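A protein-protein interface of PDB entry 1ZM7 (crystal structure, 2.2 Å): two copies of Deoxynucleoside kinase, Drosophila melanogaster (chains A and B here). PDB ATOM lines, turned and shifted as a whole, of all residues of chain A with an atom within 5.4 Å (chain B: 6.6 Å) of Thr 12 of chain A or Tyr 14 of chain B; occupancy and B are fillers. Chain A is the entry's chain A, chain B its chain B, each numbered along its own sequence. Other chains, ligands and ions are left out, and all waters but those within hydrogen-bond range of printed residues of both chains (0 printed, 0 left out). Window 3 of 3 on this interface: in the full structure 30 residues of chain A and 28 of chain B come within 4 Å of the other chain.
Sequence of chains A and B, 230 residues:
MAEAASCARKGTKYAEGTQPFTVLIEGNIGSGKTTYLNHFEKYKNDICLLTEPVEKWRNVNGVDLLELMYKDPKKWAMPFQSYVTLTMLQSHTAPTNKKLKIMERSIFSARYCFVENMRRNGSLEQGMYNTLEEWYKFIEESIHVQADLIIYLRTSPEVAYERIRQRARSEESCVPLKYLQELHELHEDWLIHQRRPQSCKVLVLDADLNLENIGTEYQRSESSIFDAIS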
ATOM      1  N   THR A  12      23.234 -24.726   8.879  1.00  0.00           N
ATOM      2  CA  THR A  12      22.927 -24.268  10.272  1.00  0.00           C
ATOM      3  C   THR A  12      21.670 -23.391  10.383  1.00  0.00           C
ATOM      4  O   THR A  12      21.638 -22.252   9.908  1.00  0.00           O
ATOM      5  CB  THR A  12      24.110 -23.507  10.869  1.00  0.00           C
ATOM      6  OG1 THR A  12      25.229 -23.574   9.970  1.00  0.00           O
ATOM      7  CG2 THR A  12      24.592 -24.206  12.137  1.00  0.00           C
ATOM      8  N   LYS A  13      20.663 -23.923  11.066  1.00  0.00           N
ATOM      9  CA  LYS A  13      19.366 -23.270  11.193  1.00  0.00           C
ATOM     10  C   LYS A  13      19.388 -22.166  12.239  1.00  0.00           C
ATOM     11  O   LYS A  13      20.134 -22.231  13.220  1.00  0.00           O
ATOM     12  CB  LYS A  13      18.284 -24.304  11.510  1.00  0.00           C
ATOM     13  CG  LYS A  13      18.268 -25.470  10.536  1.00  0.00           C
ATOM     14  CD  LYS A  13      17.186 -26.489  10.874  1.00  0.00           C
ATOM     15  CE  LYS A  13      17.248 -27.659   9.923  1.00  0.00           C
ATOM     16  NZ  LYS A  13      16.234 -28.703  10.254  1.00  0.00           N
ATOM     17  N   TYR A  14      18.571 -21.140  12.013  1.00  0.00           N
ATOM     18  CA  TYR A  14      18.348 -20.113  13.011  1.00  0.00           C
ATOM     19  C   TYR A  14      17.817 -20.719  14.323  1.00  0.00           C
ATOM     20  O   TYR A  14      17.001 -21.646  14.301  1.00  0.00           O
ATOM     21  CB  TYR A  14      17.377 -19.064  12.483  1.00  0.00           C
ATOM     22  CG  TYR A  14      17.070 -17.979  13.478  1.00  0.00           C
ATOM     23  CD1 TYR A  14      18.031 -17.030  13.814  1.00  0.00           C
ATOM     24  CD2 TYR A  14      15.817 -17.908  14.101  1.00  0.00           C
ATOM     25  CE1 TYR A  14      17.752 -16.028  14.731  1.00  0.00           C
ATOM     26  CE2 TYR A  14      15.530 -16.906  15.021  1.00  0.00           C
ATOM     27  CZ  TYR A  14      16.502 -15.968  15.321  1.00  0.00           C
ATOM     28  OH  TYR A  14      16.241 -14.971  16.233  1.00  0.00           O
ATOM     29  N   GLU A  16      19.339 -22.693  16.280  1.00  0.00           N
ATOM     30  CA  GLU A  16      20.008 -23.965  16.582  1.00  0.00           C
ATOM     31  C   GLU A  16      20.934 -23.838  17.811  1.00  0.00           C
ATOM     32  O   GLU A  16      21.720 -22.891  17.898  1.00  0.00           O
ATOM     33  CB  GLU A  16      20.807 -24.433  15.374  1.00  0.00           C
ATOM     34  CG  GLU A  16      21.302 -25.864  15.458  1.00  0.00           C
ATOM     35  CD  GLU A  16      20.870 -26.696  14.265  1.00  0.00           C
ATOM     36  OE1 GLU A  16      21.280 -26.378  13.111  1.00  0.00           O
ATOM     37  OE2 GLU A  16      20.104 -27.668  14.482  1.00  0.00           O
ATOM     38  N   PHE A 138      10.046 -24.368   3.688  1.00  0.00           N
ATOM     39  CA  PHE A 138      11.192 -23.496   3.901  1.00  0.00           C
ATOM     40  C   PHE A 138      11.553 -23.346   5.382  1.00  0.00           C
ATOM     41  O   PHE A 138      12.736 -23.264   5.728  1.00  0.00           O
ATOM     42  CB  PHE A 138      10.975 -22.112   3.302  1.00  0.00           C
ATOM     43  CG  PHE A 138      12.133 -21.188   3.497  1.00  0.00           C
ATOM     44  CD1 PHE A 138      13.315 -21.364   2.770  1.00  0.00           C
ATOM     45  CD2 PHE A 138      12.071 -20.165   4.439  1.00  0.00           C
ATOM     46  CE1 PHE A 138      14.389 -20.502   2.945  1.00  0.00           C
ATOM     47  CE2 PHE A 138      13.157 -19.315   4.628  1.00  0.00           C
ATOM     48  CZ  PHE A 138      14.305 -19.477   3.876  1.00  0.00           C
ATOM     49  N   GLU A 141      13.625 -26.201   6.746  1.00  0.00           N
ATOM     50  CA  GLU A 141      15.017 -26.156   6.303  1.00  0.00           C
ATOM     51  C   GLU A 141      15.837 -25.058   6.968  1.00  0.00           C
ATOM     52  O   GLU A 141      17.060 -25.152   7.036  1.00  0.00           O
ATOM     53  CB  GLU A 141      15.087 -26.017   4.773  1.00  0.00           C
ATOM     54  CG  GLU A 141      14.457 -27.194   4.025  1.00  0.00           C
ATOM     55  CD  GLU A 141      14.178 -26.903   2.550  1.00  0.00           C
ATOM     56  OE1 GLU A 141      13.214 -26.162   2.245  1.00  0.00           O
ATOM     57  OE2 GLU A 141      14.913 -27.433   1.679  1.00  0.00           O
ATOM     58  N   SER A 142      15.190 -24.022   7.481  1.00  0.00           N
ATOM     59  CA  SER A 142      15.934 -22.835   7.872  1.00  0.00           C
ATOM     60  C   SER A 142      15.830 -22.436   9.335  1.00  0.00           C
ATOM     61  O   SER A 142      16.668 -21.668   9.817  1.00  0.00           O
ATOM     62  CB  SER A 142      15.516 -21.646   6.992  1.00  0.00           C
ATOM     63  OG  SER A 142      14.249 -21.127   7.381  1.00  0.00           O
ATOM     64  N   THR B  12      22.875 -15.832  15.596  1.00  0.00           N
ATOM     65  CA  THR B  12      23.358 -16.327  14.267  1.00  0.00           C
ATOM     66  C   THR B  12      22.233 -16.642  13.271  1.00  0.00           C
ATOM     67  O   THR B  12      21.471 -17.604  13.444  1.00  0.00           O
ATOM     68  CB  THR B  12      24.235 -17.569  14.428  1.00  0.00           C
ATOM     69  OG1 THR B  12      24.457 -17.821  15.827  1.00  0.00           O
ATOM     70  CG2 THR B  12      25.623 -17.301  13.856  1.00  0.00           C
ATOM     71  N   LYS B  13      22.183 -15.854  12.199  1.00  0.00           N
ATOM     72  CA  LYS B  13      21.128 -15.959  11.196  1.00  0.00           C
ATOM     73  C   LYS B  13      21.362 -17.116  10.242  1.00  0.00           C
ATOM     74  O   LYS B  13      22.508 -17.488   9.960  1.00  0.00           O
ATOM     75  CB  LYS B  13      20.999 -14.641  10.435  1.00  0.00           C
ATOM     76  CG  LYS B  13      20.834 -13.433  11.354  1.00  0.00           C
ATOM     77  CD  LYS B  13      20.711 -12.130  10.571  1.00  0.00           C
ATOM     78  CE  LYS B  13      20.617 -10.955  11.518  1.00  0.00           C
ATOM     79  NZ  LYS B  13      20.546  -9.658  10.795  1.00  0.00           N
ATOM     80  N   TYR B  14      20.268 -17.694   9.756  1.00  0.00           N
ATOM     81  CA  TYR B  14      20.340 -18.680   8.691  1.00  0.00           C
ATOM     82  C   TYR B  14      21.032 -18.107   7.444  1.00  0.00           C
ATOM     83  O   TYR B  14      20.827 -16.942   7.096  1.00  0.00           O
ATOM     84  CB  TYR B  14      18.944 -19.177   8.339  1.00  0.00           C
ATOM     85  CG  TYR B  14      18.931 -20.181   7.221  1.00  0.00           C
ATOM     86  CD1 TYR B  14      19.417 -21.468   7.415  1.00  0.00           C
ATOM     87  CD2 TYR B  14      18.438 -19.839   5.951  1.00  0.00           C
ATOM     88  CE1 TYR B  14      19.410 -22.396   6.386  1.00  0.00           C
ATOM     89  CE2 TYR B  14      18.429 -20.765   4.914  1.00  0.00           C
ATOM     90  CZ  TYR B  14      18.908 -22.041   5.146  1.00  0.00           C
ATOM     91  OH  TYR B  14      18.912 -22.976   4.139  1.00  0.00           O
ATOM     92  N   ALA B  15      21.834 -18.952   6.792  1.00  0.00           N
ATOM     93  CA  ALA B  15      22.695 -18.586   5.654  1.00  0.00           C
ATOM     94  C   ALA B  15      23.877 -17.623   5.929  1.00  0.00           C
ATOM     95  O   ALA B  15      24.622 -17.289   5.001  1.00  0.00           O
ATOM     96  CB  ALA B  15      21.858 -18.097   4.454  1.00  0.00           C
ATOM     97  N   GLU B  16      24.056 -17.191   7.179  1.00  0.00           N
ATOM     98  CA  GLU B  16      25.195 -16.342   7.553  1.00  0.00           C
ATOM     99  C   GLU B  16      26.535 -16.998   7.164  1.00  0.00           C
ATOM    100  O   GLU B  16      26.751 -18.180   7.440  1.00  0.00           O
ATOM    101  CB  GLU B  16      25.166 -16.060   9.050  1.00  0.00           C
ATOM    102  CG  GLU B  16      26.113 -14.970   9.506  1.00  0.00           C
ATOM    103  CD  GLU B  16      25.402 -13.874  10.281  1.00  0.00           C
ATOM    104  OE1 GLU B  16      24.837 -14.162  11.373  1.00  0.00           O
ATOM    105  OE2 GLU B  16      25.399 -12.721   9.786  1.00  0.00           O
ATOM    106  N   THR B  18      27.573 -17.944   4.206  1.00  0.00           N
ATOM    107  CA  THR B  18      27.506 -18.902   3.095  1.00  0.00           C
ATOM    108  C   THR B  18      27.445 -18.192   1.743  1.00  0.00           C
ATOM    109  O   THR B  18      27.399 -18.839   0.697  1.00  0.00           O
ATOM    110  CB  THR B  18      26.274 -19.851   3.234  1.00  0.00           C
ATOM    111  OG1 THR B  18      25.060 -19.087   3.081  1.00  0.00           O
ATOM    112  CG2 THR B  18      26.161 -20.443   4.649  1.00  0.00           C
ATOM    113  N   LEU B  89      13.541 -15.060  -0.604  1.00  0.00           N
ATOM    114  CA  LEU B  89      14.294 -15.667   0.487  1.00  0.00           C
ATOM    115  C   LEU B  89      15.037 -16.942   0.062  1.00  0.00           C
ATOM    116  O   LEU B  89      16.193 -17.135   0.427  1.00  0.00           O
ATOM    117  CB  LEU B  89      13.357 -16.010   1.619  1.00  0.00           C
ATOM    118  CG  LEU B  89      13.626 -15.502   3.015  1.00  0.00           C
ATOM    119  CD1 LEU B  89      14.487 -14.211   3.013  1.00  0.00           C
ATOM    120  CD2 LEU B  89      12.277 -15.323   3.690  1.00  0.00           C
ATOM    121  N   THR B  93      19.145 -16.987  -0.051  1.00  0.00           N
ATOM    122  CA  THR B  93      19.859 -17.980   0.768  1.00  0.00           C
ATOM    123  C   THR B  93      20.336 -19.231   0.037  1.00  0.00           C
ATOM    124  O   THR B  93      20.931 -20.096   0.656  1.00  0.00           O
ATOM    125  CB  THR B  93      19.039 -18.425   2.006  1.00  0.00           C
ATOM    126  OG1 THR B  93      17.848 -19.088   1.586  1.00  0.00           O
ATOM    127  CG2 THR B  93      18.560 -17.239   2.812  1.00  0.00           C
ATOM    128  N   ALA B  94      20.082 -19.339  -1.261  1.00  0.00           N
ATOM    129  CA  ALA B  94      20.520 -20.516  -2.015  1.00  0.00           C
ATOM    130  C   ALA B  94      22.052 -20.676  -1.933  1.00  0.00           C
ATOM    131  O   ALA B  94      22.786 -19.686  -2.036  1.00  0.00           O
ATOM    132  CB  ALA B  94      20.053 -20.451  -3.471  1.00  0.00           C
ATOM    133  N   PRO B  95      22.524 -21.903  -1.708  1.00  0.00           N
ATOM    134  CA  PRO B  95      23.971 -22.162  -1.586  1.00  0.00           C
ATOM    135  C   PRO B  95      24.653 -22.073  -2.945  1.00  0.00           C
ATOM    136  O   PRO B  95      24.042 -22.407  -3.957  1.00  0.00           O
ATOM    137  CB  PRO B  95      24.036 -23.601  -1.056  1.00  0.00           C
ATOM    138  CG  PRO B  95      22.615 -23.913  -0.596  1.00  0.00           C
ATOM    139  CD  PRO B  95      21.730 -23.139  -1.551  1.00  0.00           C
ATOM    140  N   GLU B 141      15.613 -10.402  11.495  1.00  0.00           N
ATOM    141  CA  GLU B 141      16.265 -10.931  12.692  1.00  0.00           C
ATOM    142  C   GLU B 141      16.807 -12.348  12.524  1.00  0.00           C
ATOM    143  O   GLU B 141      17.712 -12.756  13.244  1.00  0.00           O
ATOM    144  CB  GLU B 141      15.305 -10.868  13.891  1.00  0.00           C
ATOM    145  CG  GLU B 141      14.872  -9.446  14.252  1.00  0.00           C
ATOM    146  CD  GLU B 141      13.652  -9.393  15.170  1.00  0.00           C
ATOM    147  OE1 GLU B 141      12.518  -9.639  14.694  1.00  0.00           O
ATOM    148  OE2 GLU B 141      13.814  -9.079  16.373  1.00  0.00           O
ATOM    149  N   SER B 142      16.284 -13.106  11.571  1.00  0.00           N
ATOM    150  CA  SER B 142      16.566 -14.529  11.553  1.00  0.00           C
ATOM    151  C   SER B 142      17.251 -15.058  10.304  1.00  0.00           C
ATOM    152  O   SER B 142      17.818 -16.149  10.339  1.00  0.00           O
ATOM    153  CB  SER B 142      15.266 -15.315  11.795  1.00  0.00           C
ATOM    154  OG  SER B 142      14.447 -15.346  10.631  1.00  0.00           O
ATOM    155  N   ILE B 143      17.139 -14.327   9.192  1.00  0.00           N
ATOM    156  CA  ILE B 143      17.672 -14.798   7.911  1.00  0.00           C
ATOM    157  C   ILE B 143      18.666 -13.781   7.390  1.00  0.00           C
ATOM    158  O   ILE B 143      18.381 -12.580   7.355  1.00  0.00           O
ATOM    159  CB  ILE B 143      16.549 -15.026   6.845  1.00  0.00           C
ATOM    160  CG1 ILE B 143      15.342 -15.787   7.427  1.00  0.00           C
ATOM    161  CG2 ILE B 143      17.123 -15.688   5.595  1.00  0.00           C
ATOM    162  CD1 ILE B 143      15.449 -17.309   7.419  1.00  0.00           C
ATOM    163  N   HIS B 144      19.836 -14.269   6.990  1.00  0.00           N
ATOM    164  CA  HIS B 144      20.861 -13.395   6.430  1.00  0.00           C
ATOM    165  C   HIS B 144      20.582 -13.131   4.957  1.00  0.00           C
ATOM    166  O   HIS B 144      20.438 -14.061   4.164  1.00  0.00           O
ATOM    167  CB  HIS B 144      22.270 -13.979   6.598  1.00  0.00           C
ATOM    168  CG  HIS B 144      23.338 -13.140   5.962  1.00  0.00           C
ATOM    169  ND1 HIS B 144      23.704 -11.908   6.457  1.00  0.00           N
ATOM    170  CD2 HIS B 144      24.082 -13.339   4.848  1.00  0.00           C
ATOM    171  CE1 HIS B 144      24.647 -11.391   5.687  1.00  0.00           C
ATOM    172  NE2 HIS B 144      24.895 -12.242   4.704  1.00  0.00           N
ATOM    173  N   VAL B 145      20.519 -11.851   4.614  1.00  0.00           N
ATOM    174  CA  VAL B 145      20.284 -11.427   3.241  1.00  0.00           C
ATOM    175  C   VAL B 145      21.493 -10.612   2.791  1.00  0.00           C
ATOM    176  O   VAL B 145      21.642  -9.436   3.138  1.00  0.00           O
ATOM    177  CB  VAL B 145      18.953 -10.624   3.091  1.00  0.00           C
ATOM    178  CG1 VAL B 145      18.767 -10.135   1.649  1.00  0.00           C
ATOM    179  CG2 VAL B 145      17.746 -11.475   3.541  1.00  0.00           C
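The backbone NH of Tyr 14 of chain A is in hydrogen-bond range of the backbone carbonyl oxygen of Ser 142 of chain A (3.0 Å). The backbone carbonyl oxygen (O) of Phe 138 of chain A is in hydrogen-bond range of the side-chain hydroxyl (OG) of Ser 142 of chain A. The backbone carbonyl oxygen (O) of Ser 142 of chain B lies within hydrogen-bond range of the backbone NH (N) of Tyr 14 of chain B. The backbone NH (N) of His 144 of chain B is in hydrogen-bond range of the backbone carbonyl oxygen (O) of Tyr 14 of chain B, 2.9 Å away. The backbone carbonyl oxygen of Leu 89 of chain B is in hydrogen-bond range of the side-chain hydroxyl of Thr 93 of chain B (2.8 Å).
Thr 12 of chain A touches Tyr 14 of chain B (O to CD1, 3.4 Å). CD1 of Tyr 14 of chain A touches O of Thr 12 of chain B (3.5 Å). Tyr 14 of chain A touches Glu 141 of chain B (CE1 to O, 3.6 Å). Tyr 14 of chain A touches Ser 142 of chain B. Thr 93 of chain B touches Phe 138 of chain A. Glu 141 of chain A touches Tyr 14 of chain B (O to CE1, 3.7 Å). Tyr 14 of chain B touches Ser 142 of chain A (CD2 to CB, 3.6 Å).
Printed residues of chain B within 4 Å of Tyr 14 of chain A: Thr 12, Glu 141 and Ser 142. Of the printed residues of chain B, Phe 138 of chain A touches Thr 93. Printed residues of chain B within 4 Å of Glu 141 of chain A: Tyr 14. Of the printed residues of chain A, Thr 12 of chain B touches Tyr 14 (3.5 Å). Tyr 14 of chain B touches just these residues of chain A: Thr 12 (3.4 Å), Glu 141 (3.7 Å) and Ser 142 (3.6 Å). Pro 95 of chain B touches none of the printed residues of chain A. Of the printed residues of chain A, Ser 142 of chain B touches Tyr 14 (3.5 Å). The nearest residue of chain B that does not touch Thr 12 of chain A is Ala 15 of chain B (4.5 Å). The nearest printed residue of chain A that does not touch Tyr 14 of chain B is Tyr 14 of chain A (4.2 Å).
Hydrophobic or aromatic side chains of chain B within 4 Å of the printed part of chain A: Tyr 14. Hydrophobic or aromatic side chains of chain A within 4 Å of the printed part of chain B: Tyr 14 and Phe 138. Among the printed residues, 7 pairs touch across the chains.
Thr 12 of chain A touches Tyr 14 of chain B, and with the chains exchanged Tyr 14 of chain A touches Thr 12 of chain B. Tyr 14 of chain A touches Glu 141 of chain B, and with the chains exchanged Glu 141 of chain A touches Tyr 14 of chain B. Tyr 14 of chain A touches Ser 142 of chain B, and with the chains exchanged Ser 142 of chain A touches Tyr 14 of chain B.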
